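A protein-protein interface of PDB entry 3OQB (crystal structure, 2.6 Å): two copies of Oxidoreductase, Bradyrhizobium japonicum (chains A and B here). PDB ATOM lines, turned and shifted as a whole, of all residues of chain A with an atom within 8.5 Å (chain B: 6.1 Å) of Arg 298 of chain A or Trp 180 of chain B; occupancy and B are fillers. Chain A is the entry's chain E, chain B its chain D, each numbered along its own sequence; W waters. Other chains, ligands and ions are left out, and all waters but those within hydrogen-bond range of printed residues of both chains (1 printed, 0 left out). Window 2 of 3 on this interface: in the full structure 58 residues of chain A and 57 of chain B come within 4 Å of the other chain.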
ATOM      1  N   PHE A 160     -10.474  -7.672  -4.521  1.00  0.00           N
ATOM      2  CA  PHE A 160      -9.662  -8.265  -3.470  1.00  0.00           C
ATOM      3  C   PHE A 160      -9.078  -7.259  -2.507  1.00  0.00           C
ATOM      4  O   PHE A 160      -9.024  -7.533  -1.318  1.00  0.00           O
ATOM      5  CB  PHE A 160      -8.513  -9.104  -4.031  1.00  0.00           C
ATOM      6  CG  PHE A 160      -7.565  -9.600  -2.970  1.00  0.00           C
ATOM      7  CD1 PHE A 160      -7.882 -10.733  -2.209  1.00  0.00           C
ATOM      8  CD2 PHE A 160      -6.358  -8.912  -2.702  1.00  0.00           C
ATOM      9  CE1 PHE A 160      -7.020 -11.185  -1.205  1.00  0.00           C
ATOM     10  CE2 PHE A 160      -5.479  -9.357  -1.702  1.00  0.00           C
ATOM     11  CZ  PHE A 160      -5.815 -10.499  -0.946  1.00  0.00           C
ATOM     12  N   PHE A 161      -8.617  -6.112  -3.001  1.00  0.00           N
ATOM     13  CA  PHE A 161      -7.895  -5.180  -2.146  1.00  0.00           C
ATOM     14  C   PHE A 161      -8.797  -4.296  -1.285  1.00  0.00           C
ATOM     15  O   PHE A 161      -8.381  -3.852  -0.208  1.00  0.00           O
ATOM     16  CB  PHE A 161      -6.994  -4.288  -2.971  1.00  0.00           C
ATOM     17  CG  PHE A 161      -5.865  -5.009  -3.646  1.00  0.00           C
ATOM     18  CD1 PHE A 161      -4.824  -5.546  -2.905  1.00  0.00           C
ATOM     19  CD2 PHE A 161      -5.831  -5.129  -5.026  1.00  0.00           C
ATOM     20  CE1 PHE A 161      -3.786  -6.209  -3.518  1.00  0.00           C
ATOM     21  CE2 PHE A 161      -4.782  -5.789  -5.647  1.00  0.00           C
ATOM     22  CZ  PHE A 161      -3.756  -6.329  -4.882  1.00  0.00           C
ATOM     23  N   GLY A 162     -10.026  -4.048  -1.750  1.00  0.00           N
ATOM     24  CA  GLY A 162     -10.858  -3.006  -1.176  1.00  0.00           C
ATOM     25  C   GLY A 162     -10.351  -1.689  -1.739  1.00  0.00           C
ATOM     26  O   GLY A 162     -10.431  -1.457  -2.942  1.00  0.00           O
ATOM     27  N   GLY A 281      -3.676  -3.214   0.509  1.00  0.00           N
ATOM     28  CA  GLY A 281      -5.010  -2.677   0.449  1.00  0.00           C
ATOM     29  C   GLY A 281      -5.741  -2.883   1.754  1.00  0.00           C
ATOM     30  O   GLY A 281      -5.262  -3.561   2.671  1.00  0.00           O
ATOM     31  N   THR A 282      -6.922  -2.291   1.816  1.00  0.00           N
ATOM     32  CA  THR A 282      -7.783  -2.354   2.970  1.00  0.00           C
ATOM     33  C   THR A 282      -8.183  -3.793   3.324  1.00  0.00           C
ATOM     34  O   THR A 282      -8.209  -4.160   4.488  1.00  0.00           O
ATOM     35  CB  THR A 282      -8.998  -1.408   2.748  1.00  0.00           C
ATOM     36  OG1 THR A 282      -8.690  -0.131   3.317  1.00  0.00           O
ATOM     37  CG2 THR A 282     -10.235  -1.907   3.430  1.00  0.00           C
ATOM     38  N   HIS A 283      -8.474  -4.599   2.307  1.00  0.00           N
ATOM     39  CA  HIS A 283      -9.077  -5.917   2.496  1.00  0.00           C
ATOM     40  C   HIS A 283      -8.061  -7.030   2.263  1.00  0.00           C
ATOM     41  O   HIS A 283      -8.385  -8.201   2.449  1.00  0.00           O
ATOM     42  CB  HIS A 283     -10.244  -6.125   1.522  1.00  0.00           C
ATOM     43  CG  HIS A 283     -11.458  -5.294   1.811  1.00  0.00           C
ATOM     44  ND1 HIS A 283     -11.615  -4.552   2.967  1.00  0.00           N
ATOM     45  CD2 HIS A 283     -12.606  -5.136   1.104  1.00  0.00           C
ATOM     46  CE1 HIS A 283     -12.792  -3.950   2.947  1.00  0.00           C
ATOM     47  NE2 HIS A 283     -13.412  -4.287   1.826  1.00  0.00           N
ATOM     48  N   GLY A 284      -6.852  -6.682   1.836  1.00  0.00           N
ATOM     49  CA  GLY A 284      -5.859  -7.697   1.583  1.00  0.00           C
ATOM     50  C   GLY A 284      -4.635  -7.161   0.884  1.00  0.00           C
ATOM     51  O   GLY A 284      -4.610  -6.003   0.424  1.00  0.00           O
ATOM     52  N   SER A 285      -3.607  -7.999   0.801  1.00  0.00           N
ATOM     53  CA  SER A 285      -2.368  -7.565   0.152  1.00  0.00           C
ATOM     54  C   SER A 285      -1.898  -8.622  -0.787  1.00  0.00           C
ATOM     55  O   SER A 285      -2.298  -9.783  -0.673  1.00  0.00           O
ATOM     56  CB  SER A 285      -1.269  -7.263   1.171  1.00  0.00           C
ATOM     57  OG  SER A 285      -1.616  -6.127   1.916  1.00  0.00           O
ATOM     58  N   ILE A 295      -1.088 -13.825  -1.974  1.00  0.00           N
ATOM     59  CA  ILE A 295      -2.082 -12.944  -1.375  1.00  0.00           C
ATOM     60  C   ILE A 295      -2.261 -13.234   0.106  1.00  0.00           C
ATOM     61  O   ILE A 295      -2.111 -14.386   0.565  1.00  0.00           O
ATOM     62  CB  ILE A 295      -3.482 -13.054  -2.059  1.00  0.00           C
ATOM     63  CG1 ILE A 295      -4.021 -14.483  -2.006  1.00  0.00           C
ATOM     64  CG2 ILE A 295      -3.446 -12.563  -3.504  1.00  0.00           C
ATOM     65  CD1 ILE A 295      -5.509 -14.543  -1.957  1.00  0.00           C
ATOM     66  N   GLN A 296      -2.596 -12.182   0.847  1.00  0.00           N
ATOM     67  CA  GLN A 296      -3.030 -12.334   2.219  1.00  0.00           C
ATOM     68  C   GLN A 296      -4.285 -11.481   2.448  1.00  0.00           C
ATOM     69  O   GLN A 296      -4.205 -10.265   2.598  1.00  0.00           O
ATOM     70  CB  GLN A 296      -1.902 -11.957   3.164  1.00  0.00           C
ATOM     71  CG  GLN A 296      -2.292 -11.972   4.640  1.00  0.00           C
ATOM     72  CD  GLN A 296      -1.121 -11.661   5.549  1.00  0.00           C
ATOM     73  OE1 GLN A 296      -1.113 -10.649   6.242  1.00  0.00           O
ATOM     74  NE2 GLN A 296      -0.117 -12.544   5.545  1.00  0.00           N
ATOM     75  N   ALA A 297      -5.447 -12.122   2.433  1.00  0.00           N
ATOM     76  CA  ALA A 297      -6.706 -11.457   2.773  1.00  0.00           C
ATOM     77  C   ALA A 297      -6.580 -10.882   4.156  1.00  0.00           C
ATOM     78  O   ALA A 297      -5.851 -11.412   4.979  1.00  0.00           O
ATOM     79  CB  ALA A 297      -7.833 -12.438   2.744  1.00  0.00           C
ATOM     80  N   ARG A 298      -7.310  -9.812   4.434  1.00  0.00           N
ATOM     81  CA  ARG A 298      -7.229  -9.198   5.749  1.00  0.00           C
ATOM     82  C   ARG A 298      -7.551 -10.196   6.875  1.00  0.00           C
ATOM     83  O   ARG A 298      -6.986 -10.118   7.956  1.00  0.00           O
ATOM     84  CB  ARG A 298      -8.090  -7.934   5.823  1.00  0.00           C
ATOM     85  CG  ARG A 298      -9.567  -8.141   5.842  1.00  0.00           C
ATOM     86  CD  ARG A 298     -10.220  -6.938   6.481  1.00  0.00           C
ATOM     87  NE  ARG A 298     -11.607  -6.724   6.056  1.00  0.00           N
ATOM     88  CZ  ARG A 298     -12.253  -5.564   6.175  1.00  0.00           C
ATOM     89  NH1 ARG A 298     -13.506  -5.456   5.766  1.00  0.00           N
ATOM     90  NH2 ARG A 298     -11.636  -4.503   6.706  1.00  0.00           N
ATOM     91  N   GLN A 299      -8.422 -11.161   6.585  1.00  0.00           N
ATOM     92  CA  GLN A 299      -8.853 -12.144   7.563  1.00  0.00           C
ATOM     93  C   GLN A 299      -7.722 -13.102   7.906  1.00  0.00           C
ATOM     94  O   GLN A 299      -7.756 -13.785   8.940  1.00  0.00           O
ATOM     95  CB  GLN A 299     -10.054 -12.925   7.027  1.00  0.00           C
ATOM     96  CG  GLN A 299     -11.376 -12.127   6.978  1.00  0.00           C
ATOM     97  CD  GLN A 299     -11.437 -11.127   5.826  1.00  0.00           C
ATOM     98  OE1 GLN A 299     -10.681 -11.229   4.850  1.00  0.00           O
ATOM     99  NE2 GLN A 299     -12.344 -10.147   5.934  1.00  0.00           N
ATOM    100  N   ALA A 300      -6.714 -13.149   7.044  1.00  0.00           N
ATOM    101  CA  ALA A 300      -5.624 -14.083   7.231  1.00  0.00           C
ATOM    102  C   ALA A 300      -4.442 -13.380   7.893  1.00  0.00           C
ATOM    103  O   ALA A 300      -3.406 -13.989   8.159  1.00  0.00           O
ATOM    104  CB  ALA A 300      -5.233 -14.668   5.914  1.00  0.00           C
ATOM    105  N   THR A 301      -4.594 -12.085   8.147  1.00  0.00           N
ATOM    106  CA  THR A 301      -3.490 -11.316   8.668  1.00  0.00           C
ATOM    107  C   THR A 301      -3.243 -11.761  10.092  1.00  0.00           C
ATOM    108  O   THR A 301      -4.180 -11.819  10.890  1.00  0.00           O
ATOM    109  CB  THR A 301      -3.750  -9.801   8.522  1.00  0.00           C
ATOM    110  OG1 THR A 301      -3.901  -9.475   7.128  1.00  0.00           O
ATOM    111  CG2 THR A 301      -2.600  -8.972   9.096  1.00  0.00           C
ATOM    112  N   PRO A 302      -1.991 -12.137  10.412  1.00  0.00           N
ATOM    113  CA  PRO A 302      -1.757 -12.601  11.785  1.00  0.00           C
ATOM    114  C   PRO A 302      -1.549 -11.396  12.698  1.00  0.00           C
ATOM    115  O   PRO A 302      -1.617 -10.248  12.239  1.00  0.00           O
ATOM    116  CB  PRO A 302      -0.465 -13.422  11.665  1.00  0.00           C
ATOM    117  CG  PRO A 302       0.286 -12.778  10.538  1.00  0.00           C
ATOM    118  CD  PRO A 302      -0.751 -12.158   9.601  1.00  0.00           C
ATOM    119  N   ARG A 303      -1.250 -11.654  13.965  1.00  0.00           N
ATOM    120  CA  ARG A 303      -1.068 -10.571  14.910  1.00  0.00           C
ATOM    121  C   ARG A 303       0.240 -10.673  15.678  1.00  0.00           C
ATOM    122  O   ARG A 303       0.242 -11.067  16.841  1.00  0.00           O
ATOM    123  CB  ARG A 303      -2.252 -10.528  15.880  1.00  0.00           C
ATOM    124  CG  ARG A 303      -2.092  -9.544  17.003  1.00  0.00           C
ATOM    125  CD  ARG A 303      -3.039  -9.893  18.130  1.00  0.00           C
ATOM    126  NE  ARG A 303      -2.694  -9.161  19.338  1.00  0.00           N
ATOM    127  CZ  ARG A 303      -3.225  -7.997  19.659  1.00  0.00           C
ATOM    128  NH1 ARG A 303      -2.844  -7.389  20.772  1.00  0.00           N
ATOM    129  NH2 ARG A 303      -4.139  -7.455  18.861  1.00  0.00           N
ATOM    130  N   PHE B 176      -4.016  -3.426  13.674  1.00  0.00           N
ATOM    131  CA  PHE B 176      -5.440  -3.561  13.483  1.00  0.00           C
ATOM    132  C   PHE B 176      -6.195  -2.310  13.814  1.00  0.00           C
ATOM    133  O   PHE B 176      -5.878  -1.622  14.789  1.00  0.00           O
ATOM    134  CB  PHE B 176      -5.950  -4.757  14.263  1.00  0.00           C
ATOM    135  CG  PHE B 176      -5.532  -6.017  13.663  1.00  0.00           C
ATOM    136  CD1 PHE B 176      -6.022  -6.373  12.401  1.00  0.00           C
ATOM    137  CD2 PHE B 176      -4.587  -6.812  14.289  1.00  0.00           C
ATOM    138  CE1 PHE B 176      -5.617  -7.524  11.807  1.00  0.00           C
ATOM    139  CE2 PHE B 176      -4.158  -7.987  13.684  1.00  0.00           C
ATOM    140  CZ  PHE B 176      -4.673  -8.346  12.449  1.00  0.00           C
ATOM    141  N   GLU B 177      -7.186  -2.020  12.984  1.00  0.00           N
ATOM    142  CA  GLU B 177      -7.880  -0.750  13.060  1.00  0.00           C
ATOM    143  C   GLU B 177      -8.754  -0.654  14.311  1.00  0.00           C
ATOM    144  O   GLU B 177      -9.110   0.439  14.725  1.00  0.00           O
ATOM    145  CB  GLU B 177      -8.686  -0.481  11.785  1.00  0.00           C
ATOM    146  CG  GLU B 177      -7.886  -0.561  10.473  1.00  0.00           C
ATOM    147  CD  GLU B 177      -8.048  -1.910   9.735  1.00  0.00           C
ATOM    148  OE1 GLU B 177      -7.592  -2.960  10.243  1.00  0.00           O
ATOM    149  OE2 GLU B 177      -8.633  -1.912   8.631  1.00  0.00           O
ATOM    150  N   GLY B 178      -9.072  -1.780  14.934  1.00  0.00           N
ATOM    151  CA  GLY B 178      -9.840  -1.756  16.178  1.00  0.00           C
ATOM    152  C   GLY B 178     -11.252  -2.306  16.080  1.00  0.00           C
ATOM    153  O   GLY B 178     -11.818  -2.775  17.078  1.00  0.00           O
ATOM    154  N   GLY B 179     -11.817  -2.247  14.872  1.00  0.00           N
ATOM    155  CA  GLY B 179     -13.140  -2.797  14.567  1.00  0.00           C
ATOM    156  C   GLY B 179     -13.395  -4.216  15.061  1.00  0.00           C
ATOM    157  O   GLY B 179     -14.310  -4.443  15.851  1.00  0.00           O
ATOM    158  N   TRP B 180     -12.599  -5.178  14.608  1.00  0.00           N
ATOM    159  CA  TRP B 180     -12.858  -6.565  14.971  1.00  0.00           C
ATOM    160  C   TRP B 180     -11.759  -7.163  15.829  1.00  0.00           C
ATOM    161  O   TRP B 180     -11.958  -8.168  16.500  1.00  0.00           O
ATOM    162  CB  TRP B 180     -13.106  -7.402  13.723  1.00  0.00           C
ATOM    163  CG  TRP B 180     -14.246  -6.868  12.907  1.00  0.00           C
ATOM    164  CD1 TRP B 180     -15.577  -6.925  13.221  1.00  0.00           C
ATOM    165  CD2 TRP B 180     -14.159  -6.179  11.653  1.00  0.00           C
ATOM    166  NE1 TRP B 180     -16.321  -6.323  12.241  1.00  0.00           N
ATOM    167  CE2 TRP B 180     -15.484  -5.857  11.264  1.00  0.00           C
ATOM    168  CE3 TRP B 180     -13.092  -5.807  10.817  1.00  0.00           C
ATOM    169  CZ2 TRP B 180     -15.778  -5.178  10.077  1.00  0.00           C
ATOM    170  CZ3 TRP B 180     -13.382  -5.132   9.627  1.00  0.00           C
ATOM    171  CH2 TRP B 180     -14.723  -4.822   9.273  1.00  0.00           C
ATOM    172  N   GLN B 181     -10.601  -6.524  15.823  1.00  0.00           N
ATOM    173  CA  GLN B 181      -9.479  -7.030  16.571  1.00  0.00           C
ATOM    174  C   GLN B 181      -8.859  -5.881  17.356  1.00  0.00           C
ATOM    175  O   GLN B 181      -8.919  -4.727  16.932  1.00  0.00           O
ATOM    176  CB  GLN B 181      -8.472  -7.674  15.612  1.00  0.00           C
ATOM    177  CG  GLN B 181      -9.048  -8.854  14.838  1.00  0.00           C
ATOM    178  CD  GLN B 181      -7.992  -9.654  14.104  1.00  0.00           C
ATOM    179  OE1 GLN B 181      -7.358 -10.545  14.666  1.00  0.00           O
ATOM    180  NE2 GLN B 181      -7.822  -9.357  12.832  1.00  0.00           N
ATOM    181  N   GLU B 182      -8.282  -6.189  18.507  1.00  0.00           N
ATOM    182  CA  GLU B 182      -7.714  -5.153  19.347  1.00  0.00           C
ATOM    183  C   GLU B 182      -6.484  -4.626  18.622  1.00  0.00           C
ATOM    184  O   GLU B 182      -5.729  -5.409  18.067  1.00  0.00           O
ATOM    185  CB  GLU B 182      -7.334  -5.751  20.701  1.00  0.00           C
ATOM    186  CG  GLU B 182      -7.558  -4.838  21.890  1.00  0.00           C
ATOM    187  CD  GLU B 182      -7.095  -5.482  23.197  1.00  0.00           C
ATOM    188  OE1 GLU B 182      -5.861  -5.503  23.448  1.00  0.00           O
ATOM    189  OE2 GLU B 182      -7.967  -5.963  23.968  1.00  0.00           O
ATOM    190  N   ARG B 268       1.266  -5.396   5.095  1.00  0.00           N
ATOM    191  CA  ARG B 268       1.322  -6.775   5.561  1.00  0.00           C
ATOM    192  C   ARG B 268       2.718  -7.345   5.288  1.00  0.00           C
ATOM    193  O   ARG B 268       3.407  -6.914   4.355  1.00  0.00           O
ATOM    194  CB  ARG B 268       0.200  -7.604   4.953  1.00  0.00           C
ATOM    195  CG  ARG B 268      -1.129  -7.234   5.550  1.00  0.00           C
ATOM    196  CD  ARG B 268      -2.322  -7.730   4.736  1.00  0.00           C
ATOM    197  NE  ARG B 268      -3.558  -7.193   5.299  1.00  0.00           N
ATOM    198  CZ  ARG B 268      -4.282  -6.238   4.727  1.00  0.00           C
ATOM    199  NH1 ARG B 268      -5.384  -5.804   5.328  1.00  0.00           N
ATOM    200  NH2 ARG B 268      -3.903  -5.713   3.560  1.00  0.00           N
HETATM  201  O   HOH W   1      -8.838  -4.097   7.447  1.00  0.00           O
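OE1 of Gln 296 of chain A touches CG of Arg 268 of chain B, at 3.5 Å. Arg 298 of chain A touches Trp 180 of chain B (NH2 to CZ3, 3.5 Å). Arg 298 of chain A touches Arg 268 of chain B (CB to NH1, 3.5 Å). O of Thr 301 of chain A touches CZ of Phe 176 of chain B, at 3.8 Å. Pro 302 of chain A touches Phe 176 of chain B. CE2 of Phe 176 of chain B touches CB of Arg 303 of chain A, 3.9 Å away.
Water W1 lies within hydrogen-bond range of the side-chain carboxylate of Glu 177 of chain B (2.5 Å), the guanidinium group of Arg 298 of chain A (2.9 Å) and the backbone carbonyl oxygen of Thr 282 of chain A (3.0 Å).
Ile 295 of chain A touches none of the printed residues of chain B. Of chain B, only Trp 180 (3.5 Å) and Arg 268 (3.5 Å) come within 4 Å of Arg 298 of chain A. Printed residues of chain B within 4 Å of Thr 301 of chain A: Phe 176 and Arg 268. No residue of chain A comes within 4 Å of Gly 179 of chain B. Of the printed residues of chain A, Glu 182 of chain B touches Arg 303 (2.7 Å). The nearest residue of chain A that does not touch Trp 180 of chain B is Gln 299 of chain A (6.3 Å).
No position is printed for both chains. Of the 12 pairs that touch across the chains among the printed residues, none has its exchanged pair printed and touching as well.
The guanidinium group of Arg 268 of chain B sits at hydrogen-bond distance from the backbone carbonyl oxygen of Gly 281 of chain A. NH2 of Arg 268 of chain B lies within hydrogen-bond range of OG of Ser 285 of chain A. NH2 of Arg 303 of chain A sits at hydrogen-bond distance from O of Glu 182 of chain B (2.7 Å). O of Thr 282 of chain A is in hydrogen-bond range of NH1 of Arg 268 of chain B (3.4 Å). The guanidinium group (NE) of Arg 268 of chain B is in hydrogen-bond range of the side-chain hydroxyl (OG1) of Thr 301 of chain A (2.9 Å). The guanidinium group (NH2) of Arg 268 of chain B lies close to the backbone carbonyl oxygen (O) of Gly 284 of chain A (3.2 Å).
Of the 8 printed residues of chain B, 4 touch a printed residue of chain A. Hydrophobic or aromatic side chains of chain B within 4 Å of the printed part of chain A: Phe 176 and Trp 180. Along chain B the printed residues that touch a printed residue of chain A span positions 176 to 268. Printed residues of chain A that touch a printed residue of chain B: Gly 281, Thr 282, Gly 284, Ser 285, Gln 296, Arg 298, Thr 301, Pro 302 and Arg 303. Among the printed residues, no Asp or Glu carboxylate lies within 4 Å of a Lys or Arg side-chain nitrogen of the other chain.
OG1 of Thr 301 of chain A lies within hydrogen-bond range of O of Arg 298 of chain A (3.3 Å). The backbone carbonyl oxygen of His 283 of chain A is in hydrogen-bond range of the backbone NH of Arg 298 of chain A, at 2.8 Å. N of Gln 296 of chain A sits at hydrogen-bond distance from O of Ser 285 of chain A (2.9 Å). O of Phe 161 of chain A is in hydrogen-bond range of N of Thr 282 of chain A, at 2.9 Å. OG1 of Thr 301 of chain A lies within hydrogen-bond range of O of Ala 297 of chain A. OE1 of Gln 296 of chain A lies within hydrogen-bond range of OG1 of Thr 301 of chain A, 3.2 Å away.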
